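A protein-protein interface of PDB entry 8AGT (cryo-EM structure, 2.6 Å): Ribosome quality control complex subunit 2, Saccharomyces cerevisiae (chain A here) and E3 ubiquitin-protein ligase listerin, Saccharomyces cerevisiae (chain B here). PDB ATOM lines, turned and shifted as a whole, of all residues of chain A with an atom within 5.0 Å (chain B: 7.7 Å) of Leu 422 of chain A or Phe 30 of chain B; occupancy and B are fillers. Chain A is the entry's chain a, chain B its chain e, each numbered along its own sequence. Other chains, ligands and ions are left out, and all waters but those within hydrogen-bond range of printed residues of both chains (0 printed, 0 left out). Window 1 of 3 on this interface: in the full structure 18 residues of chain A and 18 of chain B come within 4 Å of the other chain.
The side-chain hydroxyl of Tyr 29 of chain B is in hydrogen-bond range of the side-chain amino group of Lys 421 of chain A, 2.8 Å away. The side-chain amino group of Lys 421 of chain A is in hydrogen-bond range of the backbone carbonyl oxygen of Asp 191 of chain B (3.4 Å). NE2 of Gln 10 of chain B sits at hydrogen-bond distance from OE2 of Glu 426 of chain A (3.3 Å). The side-chain amino group (NZ) of Lys 429 of chain A is in salt-bridge range of the side-chain carboxylate (OD2) of Asp 31 of chain B (3.4 Å). NZ of Lys 429 of chain A lies close to NH2 of Arg 24 of chain B (3.3 Å).
NZ of Lys 429 of chain A is in salt-bridge range of OE2 of Glu 426 of chain A, 3.4 Å away. The guanidinium group of Arg 24 of chain B lies within salt-bridge range of the side-chain carboxylate of Asp 31 of chain B. The side-chain hydroxyl of Ser 26 of chain B is in hydrogen-bond range of the side-chain carboxylate of Asp 31 of chain B. The side-chain amide oxygen of Asn 28 of chain B sits close to the side-chain carboxylate of Asp 31 of chain B (3.1 Å). The side-chain carboxylate (OD1) of Asp 195 of chain B sits at hydrogen-bond distance from the side-chain hydroxyl (OH) of Tyr 29 of chain B (2.9 Å). The backbone carbonyl oxygen (O) of Asp 31 of chain B is in hydrogen-bond range of the side-chain amino group (NZ) of Lys 97 of chain B (3.0 Å).
Among the printed residues, merely in contact across the chains: Leu 422 of chain A with Gln 10 of chain B, Lys 421 of chain A with Phe 30 of chain B, Glu 426 of chain A with Asn 13 of chain B, Lys 429 of chain A with Asn 13 of chain B, Leu 422 of chain A with Asp 31 of chain B, Ser 425 of chain A with Phe 30 of chain B, Leu 422 of chain A with Phe 30 of chain B, Ile 423 of chain A with Phe 9 of chain B, Thr 418 of chain A with Phe 30 of chain B, Leu 409 of chain A with Phe 9 of chain B, Thr 418 of chain A with Tyr 29 of chain B and Met 414 of chain A with Leu 33 of chain B.
Of the printed residues of chain B, Leu 409 of chain A touches Phe 9 (3.8 Å). Leu 422 of chain A touches just these residues of chain B: Gln 10 (3.5 Å), Phe 30 (3.6 Å) and Asp 31 (3.6 Å). Of the printed residues of chain B, Glu 426 of chain A touches Gln 10 (3.3 Å) and Asn 13 (3.6 Å). Of the printed residues of chain B, Lys 429 of chain A touches Asn 13, Arg 24 and Asp 31. Of the printed residues of chain A, Gln 10 of chain B touches Leu 422 (3.5 Å) and Glu 426 (3.3 Å). Of the printed residues of chain A, Tyr 29 of chain B touches Thr 418 and Lys 421. Of the printed residues of chain A, Phe 30 of chain B touches Thr 418 (3.8 Å), Lys 421 (3.5 Å), Leu 422 (3.6 Å) and Ser 425 (3.6 Å). Asn 187 of chain B touches none of the printed residues of chain A. Glu 188 of chain B touches none of the printed residues of chain A.
Of the 12 printed residues of chain A, 9 touch a printed residue of chain B. Printed residues of chain A that touch a printed residue of chain B: Leu 409, Met 414, Thr 418, Lys 421, Leu 422, Ile 423, Ser 425, Glu 426 and Lys 429. Hydrophobic or aromatic side chains of chain A that line the printed part of chain B: Leu 409, Met 414, Leu 422 and Ile 423. Among the printed residues, 17 pairs touch across the chains.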
ATOM      1  N   LEU A 409     -10.674  -2.640 -20.965  1.00  0.00           N
ATOM      2  CA  LEU A 409     -10.895  -4.053 -20.700  1.00  0.00           C
ATOM      3  C   LEU A 409     -10.200  -4.932 -21.734  1.00  0.00           C
ATOM      4  O   LEU A 409      -9.606  -5.950 -21.385  1.00  0.00           O
ATOM      5  CB  LEU A 409     -12.389  -4.350 -20.658  1.00  0.00           C
ATOM      6  CG  LEU A 409     -13.168  -3.587 -19.588  1.00  0.00           C
ATOM      7  CD1 LEU A 409     -12.759  -4.056 -18.201  1.00  0.00           C
ATOM      8  CD2 LEU A 409     -12.947  -2.089 -19.732  1.00  0.00           C
ATOM      9  N   MET A 414      -8.780  -9.558 -20.898  1.00  0.00           N
ATOM     10  CA  MET A 414      -9.797 -10.384 -20.267  1.00  0.00           C
ATOM     11  C   MET A 414     -10.597 -11.117 -21.333  1.00  0.00           C
ATOM     12  O   MET A 414     -10.722 -10.633 -22.456  1.00  0.00           O
ATOM     13  CB  MET A 414     -10.725  -9.509 -19.430  1.00  0.00           C
ATOM     14  CG  MET A 414     -11.473 -10.249 -18.337  1.00  0.00           C
ATOM     15  SD  MET A 414     -12.695  -9.211 -17.510  1.00  0.00           S
ATOM     16  CE  MET A 414     -11.653  -7.903 -16.872  1.00  0.00           C
ATOM     17  N   THR A 418     -16.195 -12.979 -20.832  1.00  0.00           N
ATOM     18  CA  THR A 418     -16.161 -12.437 -19.484  1.00  0.00           C
ATOM     19  C   THR A 418     -16.445 -10.948 -19.500  1.00  0.00           C
ATOM     20  O   THR A 418     -17.137 -10.435 -18.625  1.00  0.00           O
ATOM     21  CB  THR A 418     -14.799 -12.665 -18.826  1.00  0.00           C
ATOM     22  OG1 THR A 418     -13.766 -12.250 -19.724  1.00  0.00           O
ATOM     23  CG2 THR A 418     -14.610 -14.135 -18.502  1.00  0.00           C
ATOM     24  N   ILE A 419     -15.915 -10.246 -20.494  1.00  0.00           N
ATOM     25  CA  ILE A 419     -16.124  -8.810 -20.578  1.00  0.00           C
ATOM     26  C   ILE A 419     -17.606  -8.548 -20.728  1.00  0.00           C
ATOM     27  O   ILE A 419     -18.159  -7.684 -20.052  1.00  0.00           O
ATOM     28  CB  ILE A 419     -15.378  -8.193 -21.776  1.00  0.00           C
ATOM     29  CG1 ILE A 419     -13.866  -8.294 -21.574  1.00  0.00           C
ATOM     30  CG2 ILE A 419     -15.762  -6.736 -21.972  1.00  0.00           C
ATOM     31  CD1 ILE A 419     -13.061  -7.811 -22.760  1.00  0.00           C
ATOM     32  N   GLU A 420     -18.268  -9.330 -21.567  1.00  0.00           N
ATOM     33  CA  GLU A 420     -19.694  -9.138 -21.782  1.00  0.00           C
ATOM     34  C   GLU A 420     -20.511  -9.374 -20.519  1.00  0.00           C
ATOM     35  O   GLU A 420     -21.462  -8.647 -20.249  1.00  0.00           O
ATOM     36  CB  GLU A 420     -20.200  -9.999 -22.936  1.00  0.00           C
ATOM     37  CG  GLU A 420     -19.666  -9.559 -24.289  1.00  0.00           C
ATOM     38  CD  GLU A 420     -20.417 -10.186 -25.445  1.00  0.00           C
ATOM     39  OE1 GLU A 420     -21.393 -10.921 -25.191  1.00  0.00           O
ATOM     40  OE2 GLU A 420     -20.034  -9.940 -26.608  1.00  0.00           O
ATOM     41  N   LYS A 421     -20.142 -10.380 -19.738  1.00  0.00           N
ATOM     42  CA  LYS A 421     -20.851 -10.637 -18.494  1.00  0.00           C
ATOM     43  C   LYS A 421     -20.718  -9.445 -17.573  1.00  0.00           C
ATOM     44  O   LYS A 421     -21.674  -9.064 -16.901  1.00  0.00           O
ATOM     45  CB  LYS A 421     -20.324 -11.894 -17.812  1.00  0.00           C
ATOM     46  CG  LYS A 421     -20.980 -13.169 -18.307  1.00  0.00           C
ATOM     47  CD  LYS A 421     -22.462 -13.191 -17.971  1.00  0.00           C
ATOM     48  CE  LYS A 421     -22.705 -13.249 -16.470  1.00  0.00           C
ATOM     49  NZ  LYS A 421     -22.242 -14.530 -15.869  1.00  0.00           N
ATOM     50  N   LEU A 422     -19.537  -8.850 -17.538  1.00  0.00           N
ATOM     51  CA  LEU A 422     -19.339  -7.667 -16.722  1.00  0.00           C
ATOM     52  C   LEU A 422     -20.226  -6.521 -17.204  1.00  0.00           C
ATOM     53  O   LEU A 422     -20.801  -5.802 -16.396  1.00  0.00           O
ATOM     54  CB  LEU A 422     -17.869  -7.259 -16.723  1.00  0.00           C
ATOM     55  CG  LEU A 422     -17.446  -6.039 -15.907  1.00  0.00           C
ATOM     56  CD1 LEU A 422     -18.023  -6.091 -14.502  1.00  0.00           C
ATOM     57  CD2 LEU A 422     -15.930  -5.938 -15.865  1.00  0.00           C
ATOM     58  N   ILE A 423     -20.354  -6.353 -18.515  1.00  0.00           N
ATOM     59  CA  ILE A 423     -21.149  -5.246 -19.030  1.00  0.00           C
ATOM     60  C   ILE A 423     -22.583  -5.423 -18.559  1.00  0.00           C
ATOM     61  O   ILE A 423     -23.224  -4.470 -18.115  1.00  0.00           O
ATOM     62  CB  ILE A 423     -21.136  -5.182 -20.571  1.00  0.00           C
ATOM     63  CG1 ILE A 423     -19.709  -5.056 -21.098  1.00  0.00           C
ATOM     64  CG2 ILE A 423     -21.976  -4.019 -21.078  1.00  0.00           C
ATOM     65  CD1 ILE A 423     -18.981  -3.832 -20.598  1.00  0.00           C
ATOM     66  N   LYS A 424     -23.078  -6.653 -18.613  1.00  0.00           N
ATOM     67  CA  LYS A 424     -24.444  -6.910 -18.194  1.00  0.00           C
ATOM     68  C   LYS A 424     -24.604  -6.579 -16.724  1.00  0.00           C
ATOM     69  O   LYS A 424     -25.590  -5.964 -16.325  1.00  0.00           O
ATOM     70  CB  LYS A 424     -24.817  -8.367 -18.445  1.00  0.00           C
ATOM     71  CG  LYS A 424     -24.789  -8.760 -19.909  1.00  0.00           C
ATOM     72  CD  LYS A 424     -25.374 -10.142 -20.133  1.00  0.00           C
ATOM     73  CE  LYS A 424     -25.374 -10.493 -21.611  1.00  0.00           C
ATOM     74  NZ  LYS A 424     -26.049 -11.793 -21.873  1.00  0.00           N
ATOM     75  N   SER A 425     -23.618  -6.958 -15.921  1.00  0.00           N
ATOM     76  CA  SER A 425     -23.687  -6.699 -14.492  1.00  0.00           C
ATOM     77  C   SER A 425     -23.721  -5.213 -14.213  1.00  0.00           C
ATOM     78  O   SER A 425     -24.468  -4.760 -13.358  1.00  0.00           O
ATOM     79  CB  SER A 425     -22.492  -7.321 -13.785  1.00  0.00           C
ATOM     80  OG  SER A 425     -22.572  -7.124 -12.386  1.00  0.00           O
ATOM     81  N   GLU A 426     -22.918  -4.449 -14.940  1.00  0.00           N
ATOM     82  CA  GLU A 426     -22.904  -3.003 -14.765  1.00  0.00           C
ATOM     83  C   GLU A 426     -24.243  -2.376 -15.121  1.00  0.00           C
ATOM     84  O   GLU A 426     -24.661  -1.413 -14.489  1.00  0.00           O
ATOM     85  CB  GLU A 426     -21.764  -2.353 -15.550  1.00  0.00           C
ATOM     86  CG  GLU A 426     -20.375  -2.698 -15.031  1.00  0.00           C
ATOM     87  CD  GLU A 426     -20.089  -2.130 -13.652  1.00  0.00           C
ATOM     88  OE1 GLU A 426     -20.631  -1.057 -13.314  1.00  0.00           O
ATOM     89  OE2 GLU A 426     -19.304  -2.753 -12.907  1.00  0.00           O
ATOM     90  N   LYS A 429     -26.310  -2.816 -12.281  1.00  0.00           N
ATOM     91  CA  LYS A 429     -25.838  -1.869 -11.277  1.00  0.00           C
ATOM     92  C   LYS A 429     -26.297  -0.460 -11.606  1.00  0.00           C
ATOM     93  O   LYS A 429     -26.378   0.389 -10.723  1.00  0.00           O
ATOM     94  CB  LYS A 429     -24.318  -1.930 -11.149  1.00  0.00           C
ATOM     95  CG  LYS A 429     -23.815  -3.208 -10.499  1.00  0.00           C
ATOM     96  CD  LYS A 429     -22.384  -3.508 -10.909  1.00  0.00           C
ATOM     97  CE  LYS A 429     -21.826  -4.702 -10.153  1.00  0.00           C
ATOM     98  NZ  LYS A 429     -20.431  -5.016 -10.571  1.00  0.00           N
ATOM     99  N   ASN B   7      -9.501  -0.506 -15.048  1.00  0.00           N
ATOM    100  CA  ASN B   7     -10.863  -0.918 -14.741  1.00  0.00           C
ATOM    101  C   ASN B   7     -11.711   0.333 -14.701  1.00  0.00           C
ATOM    102  O   ASN B   7     -12.151   0.756 -13.634  1.00  0.00           O
ATOM    103  CB  ASN B   7     -10.918  -1.626 -13.393  1.00  0.00           C
ATOM    104  CG  ASN B   7     -10.420  -3.056 -13.463  1.00  0.00           C
ATOM    105  OD1 ASN B   7     -10.533  -3.712 -14.496  1.00  0.00           O
ATOM    106  ND2 ASN B   7      -9.882  -3.551 -12.355  1.00  0.00           N
ATOM    107  N   PHE B   9     -14.744   0.858 -15.819  1.00  0.00           N
ATOM    108  CA  PHE B   9     -16.123   0.605 -15.434  1.00  0.00           C
ATOM    109  C   PHE B   9     -16.247   0.552 -13.925  1.00  0.00           C
ATOM    110  O   PHE B   9     -17.213   1.059 -13.363  1.00  0.00           O
ATOM    111  CB  PHE B   9     -16.619  -0.705 -16.034  1.00  0.00           C
ATOM    112  CG  PHE B   9     -17.152  -0.566 -17.425  1.00  0.00           C
ATOM    113  CD1 PHE B   9     -18.427  -0.081 -17.640  1.00  0.00           C
ATOM    114  CD2 PHE B   9     -16.380  -0.920 -18.516  1.00  0.00           C
ATOM    115  CE1 PHE B   9     -18.927   0.050 -18.919  1.00  0.00           C
ATOM    116  CE2 PHE B   9     -16.872  -0.793 -19.799  1.00  0.00           C
ATOM    117  CZ  PHE B   9     -18.147  -0.305 -20.002  1.00  0.00           C
ATOM    118  N   GLN B  10     -15.277  -0.067 -13.266  1.00  0.00           N
ATOM    119  CA  GLN B  10     -15.297  -0.142 -11.811  1.00  0.00           C
ATOM    120  C   GLN B  10     -15.197   1.237 -11.176  1.00  0.00           C
ATOM    121  O   GLN B  10     -15.840   1.508 -10.161  1.00  0.00           O
ATOM    122  CB  GLN B  10     -14.198  -1.069 -11.294  1.00  0.00           C
ATOM    123  CG  GLN B  10     -14.241  -2.464 -11.901  1.00  0.00           C
ATOM    124  CD  GLN B  10     -15.612  -3.111 -11.806  1.00  0.00           C
ATOM    125  OE1 GLN B  10     -16.230  -3.141 -10.742  1.00  0.00           O
ATOM    126  NE2 GLN B  10     -16.086  -3.644 -12.924  1.00  0.00           N
ATOM    127  N   ASN B  13     -18.485   2.644 -11.335  1.00  0.00           N
ATOM    128  CA  ASN B  13     -19.394   1.955 -10.422  1.00  0.00           C
ATOM    129  C   ASN B  13     -19.337   2.533  -9.017  1.00  0.00           C
ATOM    130  O   ASN B  13     -20.370   2.621  -8.353  1.00  0.00           O
ATOM    131  CB  ASN B  13     -19.044   0.464 -10.385  1.00  0.00           C
ATOM    132  CG  ASN B  13     -20.158  -0.389  -9.815  1.00  0.00           C
ATOM    133  OD1 ASN B  13     -21.326  -0.002  -9.827  1.00  0.00           O
ATOM    134  ND2 ASN B  13     -19.801  -1.571  -9.325  1.00  0.00           N
ATOM    135  N   ARG B  24     -12.292  -2.981  -4.486  1.00  0.00           N
ATOM    136  CA  ARG B  24     -13.522  -3.733  -4.605  1.00  0.00           C
ATOM    137  C   ARG B  24     -13.228  -5.208  -4.486  1.00  0.00           C
ATOM    138  O   ARG B  24     -12.348  -5.726  -5.167  1.00  0.00           O
ATOM    139  CB  ARG B  24     -14.227  -3.439  -5.928  1.00  0.00           C
ATOM    140  CG  ARG B  24     -15.422  -4.339  -6.191  1.00  0.00           C
ATOM    141  CD  ARG B  24     -16.228  -3.886  -7.395  1.00  0.00           C
ATOM    142  NE  ARG B  24     -17.287  -4.838  -7.719  1.00  0.00           N
ATOM    143  CZ  ARG B  24     -18.492  -4.838  -7.159  1.00  0.00           C
ATOM    144  NH1 ARG B  24     -18.799  -3.934  -6.239  1.00  0.00           N
ATOM    145  NH2 ARG B  24     -19.391  -5.745  -7.513  1.00  0.00           N
ATOM    146  N   SER B  26     -15.177  -8.852  -4.764  1.00  0.00           N
ATOM    147  CA  SER B  26     -16.424  -9.528  -5.083  1.00  0.00           C
ATOM    148  C   SER B  26     -16.210 -10.984  -5.447  1.00  0.00           C
ATOM    149  O   SER B  26     -15.199 -11.335  -6.051  1.00  0.00           O
ATOM    150  CB  SER B  26     -17.149  -8.806  -6.217  1.00  0.00           C
ATOM    151  OG  SER B  26     -16.291  -8.645  -7.327  1.00  0.00           O
ATOM    152  N   LEU B  27     -17.158 -11.833  -5.085  1.00  0.00           N
ATOM    153  CA  LEU B  27     -17.064 -13.250  -5.405  1.00  0.00           C
ATOM    154  C   LEU B  27     -17.121 -13.536  -6.902  1.00  0.00           C
ATOM    155  O   LEU B  27     -16.438 -14.435  -7.385  1.00  0.00           O
ATOM    156  CB  LEU B  27     -18.135 -14.029  -4.652  1.00  0.00           C
ATOM    157  CG  LEU B  27     -18.238 -13.689  -3.162  1.00  0.00           C
ATOM    158  CD1 LEU B  27     -19.339 -14.499  -2.504  1.00  0.00           C
ATOM    159  CD2 LEU B  27     -16.916 -13.894  -2.437  1.00  0.00           C
ATOM    160  N   ASN B  28     -17.932 -12.783  -7.640  1.00  0.00           N
ATOM    161  CA  ASN B  28     -18.114 -13.047  -9.075  1.00  0.00           C
ATOM    162  C   ASN B  28     -16.866 -12.923  -9.938  1.00  0.00           C
ATOM    163  O   ASN B  28     -16.033 -12.056  -9.710  1.00  0.00           O
ATOM    164  CB  ASN B  28     -19.232 -12.167  -9.646  1.00  0.00           C
ATOM    165  CG  ASN B  28     -19.139 -10.719  -9.196  1.00  0.00           C
ATOM    166  OD1 ASN B  28     -18.129 -10.280  -8.649  1.00  0.00           O
ATOM    167  ND2 ASN B  28     -20.206  -9.966  -9.430  1.00  0.00           N
ATOM    168  N   TYR B  29     -16.735 -13.798 -10.929  1.00  0.00           N
ATOM    169  CA  TYR B  29     -15.543 -13.796 -11.778  1.00  0.00           C
ATOM    170  C   TYR B  29     -15.322 -12.544 -12.611  1.00  0.00           C
ATOM    171  O   TYR B  29     -14.190 -12.088 -12.743  1.00  0.00           O
ATOM    172  CB  TYR B  29     -15.498 -15.049 -12.667  1.00  0.00           C
ATOM    173  CG  TYR B  29     -16.615 -15.182 -13.681  1.00  0.00           C
ATOM    174  CD1 TYR B  29     -17.841 -15.719 -13.325  1.00  0.00           C
ATOM    175  CD2 TYR B  29     -16.429 -14.802 -15.004  1.00  0.00           C
ATOM    176  CE1 TYR B  29     -18.860 -15.847 -14.244  1.00  0.00           C
ATOM    177  CE2 TYR B  29     -17.442 -14.930 -15.932  1.00  0.00           C
ATOM    178  CZ  TYR B  29     -18.654 -15.454 -15.545  1.00  0.00           C
ATOM    179  OH  TYR B  29     -19.665 -15.591 -16.461  1.00  0.00           O
ATOM    180  N   PHE B  30     -16.381 -11.976 -13.171  1.00  0.00           N
ATOM    181  CA  PHE B  30     -16.207 -10.831 -14.069  1.00  0.00           C
ATOM    182  C   PHE B  30     -15.596  -9.576 -13.440  1.00  0.00           C
ATOM    183  O   PHE B  30     -14.792  -8.898 -14.073  1.00  0.00           O
ATOM    184  CB  PHE B  30     -17.479 -10.515 -14.870  1.00  0.00           C
ATOM    185  CG  PHE B  30     -18.754 -10.868 -14.170  1.00  0.00           C
ATOM    186  CD1 PHE B  30     -19.303 -12.130 -14.298  1.00  0.00           C
ATOM    187  CD2 PHE B  30     -19.421  -9.928 -13.414  1.00  0.00           C
ATOM    188  CE1 PHE B  30     -20.479 -12.456 -13.660  1.00  0.00           C
ATOM    189  CE2 PHE B  30     -20.600 -10.245 -12.776  1.00  0.00           C
ATOM    190  CZ  PHE B  30     -21.132 -11.510 -12.900  1.00  0.00           C
ATOM    191  N   ASP B  31     -15.962  -9.268 -12.203  1.00  0.00           N
ATOM    192  CA  ASP B  31     -15.431  -8.075 -11.547  1.00  0.00           C
ATOM    193  C   ASP B  31     -14.744  -8.391 -10.232  1.00  0.00           C
ATOM    194  O   ASP B  31     -14.943  -9.462  -9.671  1.00  0.00           O
ATOM    195  CB  ASP B  31     -16.496  -6.988 -11.366  1.00  0.00           C
ATOM    196  CG  ASP B  31     -17.680  -7.451 -10.547  1.00  0.00           C
ATOM    197  OD1 ASP B  31     -17.636  -7.327  -9.309  1.00  0.00           O
ATOM    198  OD2 ASP B  31     -18.668  -7.917 -11.144  1.00  0.00           O
ATOM    199  N   GLY B  32     -13.923  -7.472  -9.744  1.00  0.00           N
ATOM    200  CA  GLY B  32     -13.172  -7.726  -8.527  1.00  0.00           C
ATOM    201  C   GLY B  32     -11.811  -8.305  -8.826  1.00  0.00           C
ATOM    202  O   GLY B  32     -11.057  -8.621  -7.907  1.00  0.00           O
ATOM    203  N   LEU B  33     -11.485  -8.455 -10.103  1.00  0.00           N
ATOM    204  CA  LEU B  33     -10.157  -8.918 -10.481  1.00  0.00           C
ATOM    205  C   LEU B  33      -9.156  -7.829 -10.127  1.00  0.00           C
ATOM    206  O   LEU B  33      -9.476  -6.643 -10.211  1.00  0.00           O
ATOM    207  CB  LEU B  33     -10.118  -9.210 -11.977  1.00  0.00           C
ATOM    208  CG  LEU B  33     -10.913 -10.437 -12.416  1.00  0.00           C
ATOM    209  CD1 LEU B  33     -11.115 -10.442 -13.922  1.00  0.00           C
ATOM    210  CD2 LEU B  33     -10.202 -11.703 -11.963  1.00  0.00           C
ATOM    211  N   LYS B  97     -12.229 -14.772  -4.549  1.00  0.00           N
ATOM    212  CA  LYS B  97     -12.450 -15.740  -5.609  1.00  0.00           C
ATOM    213  C   LYS B  97     -11.914 -17.104  -5.221  1.00  0.00           C
ATOM    214  O   LYS B  97     -12.530 -18.126  -5.509  1.00  0.00           O
ATOM    215  CB  LYS B  97     -11.847 -15.246  -6.917  1.00  0.00           C
ATOM    216  CG  LYS B  97     -12.544 -14.005  -7.444  1.00  0.00           C
ATOM    217  CD  LYS B  97     -11.925 -13.509  -8.737  1.00  0.00           C
ATOM    218  CE  LYS B  97     -12.734 -12.351  -9.294  1.00  0.00           C
ATOM    219  NZ  LYS B  97     -13.010 -11.333  -8.246  1.00  0.00           N
ATOM    220  N   ASN B 187     -26.925 -10.560  -3.765  1.00  0.00           N
ATOM    221  CA  ASN B 187     -26.164 -10.065  -4.908  1.00  0.00           C
ATOM    222  C   ASN B 187     -25.664 -11.190  -5.796  1.00  0.00           C
ATOM    223  O   ASN B 187     -25.740 -11.105  -7.020  1.00  0.00           O
ATOM    224  CB  ASN B 187     -24.994  -9.200  -4.439  1.00  0.00           C
ATOM    225  CG  ASN B 187     -25.436  -8.038  -3.571  1.00  0.00           C
ATOM    226  OD1 ASN B 187     -26.631  -7.804  -3.385  1.00  0.00           O
ATOM    227  ND2 ASN B 187     -24.471  -7.300  -3.036  1.00  0.00           N
ATOM    228  N   GLU B 188     -25.156 -12.249  -5.183  1.00  0.00           N
ATOM    229  CA  GLU B 188     -24.634 -13.367  -5.953  1.00  0.00           C
ATOM    230  C   GLU B 188     -25.703 -14.244  -6.574  1.00  0.00           C
ATOM    231  O   GLU B 188     -26.771 -14.432  -5.994  1.00  0.00           O
ATOM    232  CB  GLU B 188     -23.670 -14.205  -5.112  1.00  0.00           C
ATOM    233  CG  GLU B 188     -22.483 -13.423  -4.565  1.00  0.00           C
ATOM    234  CD  GLU B 188     -21.564 -12.883  -5.648  1.00  0.00           C
ATOM    235  OE1 GLU B 188     -21.455 -13.512  -6.721  1.00  0.00           O
ATOM    236  OE2 GLU B 188     -20.930 -11.832  -5.415  1.00  0.00           O
ATOM    237  N   ASN B 189     -25.419 -14.783  -7.750  1.00  0.00           N
ATOM    238  CA  ASN B 189     -26.352 -15.674  -8.424  1.00  0.00           C
ATOM    239  C   ASN B 189     -25.504 -16.822  -8.912  1.00  0.00           C
ATOM    240  O   ASN B 189     -24.285 -16.710  -8.960  1.00  0.00           O
ATOM    241  CB  ASN B 189     -27.023 -14.982  -9.606  1.00  0.00           C
ATOM    242  CG  ASN B 189     -28.108 -14.015  -9.178  1.00  0.00           C
ATOM    243  OD1 ASN B 189     -28.319 -12.981  -9.812  1.00  0.00           O
ATOM    244  ND2 ASN B 189     -28.802 -14.344  -8.095  1.00  0.00           N
ATOM    245  N   ASP B 191     -25.096 -17.949 -11.794  1.00  0.00           N
ATOM    246  CA  ASP B 191     -24.368 -17.516 -12.979  1.00  0.00           C
ATOM    247  C   ASP B 191     -23.153 -16.661 -12.642  1.00  0.00           C
ATOM    248  O   ASP B 191     -22.109 -16.787 -13.273  1.00  0.00           O
ATOM    249  CB  ASP B 191     -25.298 -16.752 -13.918  1.00  0.00           C
ATOM    250  CG  ASP B 191     -26.426 -17.614 -14.442  1.00  0.00           C
ATOM    251  OD1 ASP B 191     -26.390 -18.843 -14.218  1.00  0.00           O
ATOM    252  OD2 ASP B 191     -27.347 -17.067 -15.082  1.00  0.00           O
ATOM    253  N   THR B 192     -23.285 -15.768 -11.670  1.00  0.00           N
ATOM    254  CA  THR B 192     -22.139 -14.967 -11.265  1.00  0.00           C
ATOM    255  C   THR B 192     -21.030 -15.827 -10.672  1.00  0.00           C
ATOM    256  O   THR B 192     -19.858 -15.594 -10.938  1.00  0.00           O
ATOM    257  CB  THR B 192     -22.531 -13.876 -10.257  1.00  0.00           C
ATOM    258  OG1 THR B 192     -22.791 -14.466  -8.979  1.00  0.00           O
ATOM    259  CG2 THR B 192     -23.764 -13.127 -10.732  1.00  0.00           C
ATOM    260  N   ILE B 193     -21.395 -16.803  -9.850  1.00  0.00           N
ATOM    261  CA  ILE B 193     -20.403 -17.686  -9.251  1.00  0.00           C
ATOM    262  C   ILE B 193     -19.671 -18.545 -10.273  1.00  0.00           C
ATOM    263  O   ILE B 193     -18.447 -18.675 -10.218  1.00  0.00           O
ATOM    264  CB  ILE B 193     -21.052 -18.602  -8.197  1.00  0.00           C
ATOM    265  CG1 ILE B 193     -21.717 -17.765  -7.106  1.00  0.00           C
ATOM    266  CG2 ILE B 193     -20.028 -19.536  -7.573  1.00  0.00           C
ATOM    267  CD1 ILE B 193     -20.751 -16.887  -6.340  1.00  0.00           C
ATOM    268  N   SER B 194     -20.401 -19.104 -11.230  1.00  0.00           N
ATOM    269  CA  SER B 194     -19.779 -20.015 -12.190  1.00  0.00           C
ATOM    270  C   SER B 194     -19.971 -19.571 -13.628  1.00  0.00           C
ATOM    271  O   SER B 194     -21.087 -19.278 -14.044  1.00  0.00           O
ATOM    272  CB  SER B 194     -20.370 -21.409 -12.025  1.00  0.00           C
ATOM    273  OG  SER B 194     -20.690 -21.665 -10.671  1.00  0.00           O
ATOM    274  N   ASP B 195     -18.893 -19.561 -14.405  1.00  0.00           N
ATOM    275  CA  ASP B 195     -18.993 -19.118 -15.786  1.00  0.00           C
ATOM    276  C   ASP B 195     -19.912 -20.037 -16.560  1.00  0.00           C
ATOM    277  O   ASP B 195     -19.805 -21.254 -16.465  1.00  0.00           O
ATOM    278  CB  ASP B 195     -17.619 -19.077 -16.448  1.00  0.00           C
ATOM    279  CG  ASP B 195     -17.661 -18.482 -17.843  1.00  0.00           C
ATOM    280  OD1 ASP B 195     -18.546 -17.646 -18.121  1.00  0.00           O
ATOM    281  OD2 ASP B 195     -16.803 -18.848 -18.664  1.00  0.00           O
